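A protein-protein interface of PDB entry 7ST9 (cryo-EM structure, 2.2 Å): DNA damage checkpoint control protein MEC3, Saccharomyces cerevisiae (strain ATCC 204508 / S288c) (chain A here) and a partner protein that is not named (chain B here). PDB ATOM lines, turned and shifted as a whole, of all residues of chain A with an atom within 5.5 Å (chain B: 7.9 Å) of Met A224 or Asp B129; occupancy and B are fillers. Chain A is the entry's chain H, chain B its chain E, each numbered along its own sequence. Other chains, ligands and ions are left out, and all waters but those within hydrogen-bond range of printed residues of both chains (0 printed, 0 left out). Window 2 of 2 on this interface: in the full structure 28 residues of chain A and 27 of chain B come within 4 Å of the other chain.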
ATOM      1  N   GLU A 222     -10.902  18.247  -9.862  1.00  0.00           N
ATOM      2  CA  GLU A 222     -10.209  17.236 -10.644  1.00  0.00           C
ATOM      3  C   GLU A 222     -10.669  17.287 -12.100  1.00  0.00           C
ATOM      4  O   GLU A 222     -11.868  17.422 -12.366  1.00  0.00           O
ATOM      5  CB  GLU A 222     -10.470  15.846 -10.065  1.00  0.00           C
ATOM      6  CG  GLU A 222      -9.652  14.743 -10.714  1.00  0.00           C
ATOM      7  CD  GLU A 222      -9.513  13.524  -9.826  1.00  0.00           C
ATOM      8  OE1 GLU A 222     -10.542  12.877  -9.537  1.00  0.00           O
ATOM      9  OE2 GLU A 222      -8.376  13.211  -9.416  1.00  0.00           O
ATOM     10  N   PRO A 223      -9.751  17.187 -13.064  1.00  0.00           N
ATOM     11  CA  PRO A 223     -10.175  17.155 -14.468  1.00  0.00           C
ATOM     12  C   PRO A 223     -11.068  15.958 -14.752  1.00  0.00           C
ATOM     13  O   PRO A 223     -10.886  14.872 -14.198  1.00  0.00           O
ATOM     14  CB  PRO A 223      -8.852  17.065 -15.240  1.00  0.00           C
ATOM     15  CG  PRO A 223      -7.818  17.556 -14.299  1.00  0.00           C
ATOM     16  CD  PRO A 223      -8.284  17.161 -12.937  1.00  0.00           C
ATOM     17  N   MET A 224     -12.042  16.170 -15.633  1.00  0.00           N
ATOM     18  CA  MET A 224     -12.961  15.126 -16.067  1.00  0.00           C
ATOM     19  C   MET A 224     -12.775  14.896 -17.558  1.00  0.00           C
ATOM     20  O   MET A 224     -12.742  15.854 -18.338  1.00  0.00           O
ATOM     21  CB  MET A 224     -14.413  15.508 -15.762  1.00  0.00           C
ATOM     22  CG  MET A 224     -14.675  15.805 -14.294  1.00  0.00           C
ATOM     23  SD  MET A 224     -16.375  15.458 -13.805  1.00  0.00           S
ATOM     24  CE  MET A 224     -16.491  16.408 -12.291  1.00  0.00           C
ATOM     25  N   ILE A 225     -12.656  13.631 -17.950  1.00  0.00           N
ATOM     26  CA  ILE A 225     -12.406  13.256 -19.335  1.00  0.00           C
ATOM     27  C   ILE A 225     -13.664  12.623 -19.908  1.00  0.00           C
ATOM     28  O   ILE A 225     -14.485  12.049 -19.184  1.00  0.00           O
ATOM     29  CB  ILE A 225     -11.207  12.291 -19.461  1.00  0.00           C
ATOM     30  CG1 ILE A 225     -10.035  12.762 -18.596  1.00  0.00           C
ATOM     31  CG2 ILE A 225     -10.774  12.177 -20.915  1.00  0.00           C
ATOM     32  CD1 ILE A 225      -9.568  14.172 -18.897  1.00  0.00           C
ATOM     33  N   ASN A 226     -13.812  12.731 -21.227  1.00  0.00           N
ATOM     34  CA  ASN A 226     -14.941  12.138 -21.941  1.00  0.00           C
ATOM     35  C   ASN A 226     -14.711  10.633 -22.004  1.00  0.00           C
ATOM     36  O   ASN A 226     -14.011  10.122 -22.877  1.00  0.00           O
ATOM     37  CB  ASN A 226     -15.076  12.747 -23.331  1.00  0.00           C
ATOM     38  CG  ASN A 226     -16.404  12.425 -23.981  1.00  0.00           C
ATOM     39  OD1 ASN A 226     -17.153  11.578 -23.497  1.00  0.00           O
ATOM     40  ND2 ASN A 226     -16.704  13.100 -25.085  1.00  0.00           N
ATOM     41  N   MET A 394     -12.232  26.021 -27.557  1.00  0.00           N
ATOM     42  CA  MET A 394     -12.004  24.584 -27.567  1.00  0.00           C
ATOM     43  C   MET A 394     -10.853  24.236 -28.501  1.00  0.00           C
ATOM     44  O   MET A 394     -10.764  24.747 -29.621  1.00  0.00           O
ATOM     45  CB  MET A 394     -13.269  23.845 -28.002  1.00  0.00           C
ATOM     46  CG  MET A 394     -14.367  23.819 -26.949  1.00  0.00           C
ATOM     47  SD  MET A 394     -13.921  22.875 -25.478  1.00  0.00           S
ATOM     48  CE  MET A 394     -13.733  21.230 -26.164  1.00  0.00           C
ATOM     49  N   TYR A 467      -3.032  13.290 -15.128  1.00  0.00           N
ATOM     50  CA  TYR A 467      -3.569  13.783 -16.387  1.00  0.00           C
ATOM     51  C   TYR A 467      -2.503  14.612 -17.090  1.00  0.00           C
ATOM     52  O   TYR A 467      -1.895  15.496 -16.475  1.00  0.00           O
ATOM     53  CB  TYR A 467      -4.820  14.633 -16.160  1.00  0.00           C
ATOM     54  CG  TYR A 467      -5.876  13.979 -15.298  1.00  0.00           C
ATOM     55  CD1 TYR A 467      -5.793  14.021 -13.914  1.00  0.00           C
ATOM     56  CD2 TYR A 467      -6.963  13.333 -15.870  1.00  0.00           C
ATOM     57  CE1 TYR A 467      -6.756  13.430 -13.122  1.00  0.00           C
ATOM     58  CE2 TYR A 467      -7.933  12.739 -15.086  1.00  0.00           C
ATOM     59  CZ  TYR A 467      -7.825  12.791 -13.713  1.00  0.00           C
ATOM     60  OH  TYR A 467      -8.787  12.200 -12.928  1.00  0.00           O
ATOM     61  N   PHE B 124      -6.743  22.148 -18.808  1.00  0.00           N
ATOM     62  CA  PHE B 124      -7.931  21.367 -18.494  1.00  0.00           C
ATOM     63  C   PHE B 124      -9.074  22.290 -18.092  1.00  0.00           C
ATOM     64  O   PHE B 124      -8.890  23.235 -17.319  1.00  0.00           O
ATOM     65  CB  PHE B 124      -7.636  20.377 -17.368  1.00  0.00           C
ATOM     66  CG  PHE B 124      -6.689  19.278 -17.758  1.00  0.00           C
ATOM     67  CD1 PHE B 124      -7.107  18.246 -18.581  1.00  0.00           C
ATOM     68  CD2 PHE B 124      -5.383  19.276 -17.299  1.00  0.00           C
ATOM     69  CE1 PHE B 124      -6.238  17.233 -18.941  1.00  0.00           C
ATOM     70  CE2 PHE B 124      -4.510  18.266 -17.656  1.00  0.00           C
ATOM     71  CZ  PHE B 124      -4.938  17.244 -18.478  1.00  0.00           C
ATOM     72  N   GLN B 125     -10.262  22.012 -18.622  1.00  0.00           N
ATOM     73  CA  GLN B 125     -11.438  22.809 -18.303  1.00  0.00           C
ATOM     74  C   GLN B 125     -11.962  22.434 -16.923  1.00  0.00           C
ATOM     75  O   GLN B 125     -12.138  21.250 -16.616  1.00  0.00           O
ATOM     76  CB  GLN B 125     -12.523  22.604 -19.359  1.00  0.00           C
ATOM     77  CG  GLN B 125     -12.297  23.402 -20.632  1.00  0.00           C
ATOM     78  CD  GLN B 125     -13.411  23.219 -21.641  1.00  0.00           C
ATOM     79  OE1 GLN B 125     -14.062  24.182 -22.047  1.00  0.00           O
ATOM     80  NE2 GLN B 125     -13.636  21.978 -22.054  1.00  0.00           N
ATOM     81  N   ASP B 126     -12.209  23.447 -16.090  1.00  0.00           N
ATOM     82  CA  ASP B 126     -12.657  23.190 -14.726  1.00  0.00           C
ATOM     83  C   ASP B 126     -14.027  22.523 -14.706  1.00  0.00           C
ATOM     84  O   ASP B 126     -14.263  21.595 -13.924  1.00  0.00           O
ATOM     85  CB  ASP B 126     -12.687  24.495 -13.932  1.00  0.00           C
ATOM     86  CG  ASP B 126     -12.596  24.270 -12.435  1.00  0.00           C
ATOM     87  OD1 ASP B 126     -11.723  23.489 -12.001  1.00  0.00           O
ATOM     88  OD2 ASP B 126     -13.398  24.875 -11.692  1.00  0.00           O
ATOM     89  N   SER B 127     -14.943  22.978 -15.560  1.00  0.00           N
ATOM     90  CA  SER B 127     -16.315  22.485 -15.583  1.00  0.00           C
ATOM     91  C   SER B 127     -16.629  21.663 -16.824  1.00  0.00           C
ATOM     92  O   SER B 127     -17.078  20.518 -16.710  1.00  0.00           O
ATOM     93  CB  SER B 127     -17.293  23.665 -15.487  1.00  0.00           C
ATOM     94  OG  SER B 127     -18.636  23.217 -15.507  1.00  0.00           O
ATOM     95  N   LYS B 128     -16.403  22.216 -18.012  1.00  0.00           N
ATOM     96  CA  LYS B 128     -16.719  21.517 -19.245  1.00  0.00           C
ATOM     97  C   LYS B 128     -15.693  20.419 -19.518  1.00  0.00           C
ATOM     98  O   LYS B 128     -14.626  20.353 -18.902  1.00  0.00           O
ATOM     99  CB  LYS B 128     -16.772  22.496 -20.416  1.00  0.00           C
ATOM    100  CG  LYS B 128     -17.825  23.583 -20.270  1.00  0.00           C
ATOM    101  CD  LYS B 128     -17.727  24.604 -21.393  1.00  0.00           C
ATOM    102  CE  LYS B 128     -18.668  25.776 -21.165  1.00  0.00           C
ATOM    103  NZ  LYS B 128     -18.547  26.806 -22.233  1.00  0.00           N
ATOM    104  N   ASP B 129     -16.034  19.544 -20.461  1.00  0.00           N
ATOM    105  CA  ASP B 129     -15.158  18.454 -20.861  1.00  0.00           C
ATOM    106  C   ASP B 129     -14.262  18.896 -22.010  1.00  0.00           C
ATOM    107  O   ASP B 129     -14.676  19.676 -22.872  1.00  0.00           O
ATOM    108  CB  ASP B 129     -15.975  17.229 -21.277  1.00  0.00           C
ATOM    109  CG  ASP B 129     -16.651  16.552 -20.101  1.00  0.00           C
ATOM    110  OD1 ASP B 129     -16.277  16.847 -18.946  1.00  0.00           O
ATOM    111  OD2 ASP B 129     -17.559  15.726 -20.331  1.00  0.00           O
ATOM    112  N   GLY B 130     -13.034  18.393 -22.015  1.00  0.00           N
ATOM    113  CA  GLY B 130     -12.071  18.733 -23.040  1.00  0.00           C
ATOM    114  C   GLY B 130     -11.188  19.904 -22.643  1.00  0.00           C
ATOM    115  O   GLY B 130     -11.461  20.642 -21.698  1.00  0.00           O
ATOM    116  N   LEU B 131     -10.102  20.065 -23.391  1.00  0.00           N
ATOM    117  CA  LEU B 131      -9.153  21.132 -23.124  1.00  0.00           C
ATOM    118  C   LEU B 131      -9.686  22.469 -23.633  1.00  0.00           C
ATOM    119  O   LEU B 131     -10.591  22.534 -24.469  1.00  0.00           O
ATOM    120  CB  LEU B 131      -7.803  20.834 -23.777  1.00  0.00           C
ATOM    121  CG  LEU B 131      -7.153  19.497 -23.421  1.00  0.00           C
ATOM    122  CD1 LEU B 131      -5.905  19.282 -24.261  1.00  0.00           C
ATOM    123  CD2 LEU B 131      -6.822  19.433 -21.938  1.00  0.00           C
ATOM    124  N   ALA B 132      -9.106  23.546 -23.109  1.00  0.00           N
ATOM    125  CA  ALA B 132      -9.406  24.902 -23.540  1.00  0.00           C
ATOM    126  C   ALA B 132      -8.102  25.600 -23.892  1.00  0.00           C
ATOM    127  O   ALA B 132      -7.099  25.449 -23.188  1.00  0.00           O
ATOM    128  CB  ALA B 132     -10.150  25.685 -22.454  1.00  0.00           C
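NE2 of Gln B125 lies within hydrogen-bond range of SD of Met A394 (3.6 Å). The side-chain sulfur of Met A394 sits close to the backbone carbonyl oxygen of Leu B131.
NE2 of Gln B125 sits at hydrogen-bond distance from O of Asp B129, at 2.7 Å. NE2 of Gln B125 sits at hydrogen-bond distance from O of Gly B130, 2.6 Å away.
Among the printed residues, pairs that only touch across the chains: Tyr A467 with Phe B124, Met A224 with Asp B129, Met A394 with Asp B129 and Pro A223 with Phe B124.
Of the printed residues of chain B, Pro A223 touches Phe B124 (3.9 Å). Asn A226 touches none of the printed residues of chain B. Of the printed residues of chain A, Gln B125 touches Met A394. Of chain A, only Met A224 (3.7 Å) and Met A394 (3.8 Å) come within 4 Å of Asp B129. Printed residues of chain A within 4 Å of Leu B131: Met A394 (3.5 Å). The nearest residue of chain A that does not touch Asp B129 is Asn A226 (4.7 Å). The nearest printed residue of chain A that does not touch Gln B125 is Pro A223 (5.0 Å).
Of the 9 printed residues of chain B, 4 touch a printed residue of chain A. Of the 7 printed residues of chain A, 4 touch a printed residue of chain B. Among the printed residues, no Asp or Glu carboxylate lies within 4 Å of a Lys or Arg side-chain nitrogen of the other chain.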
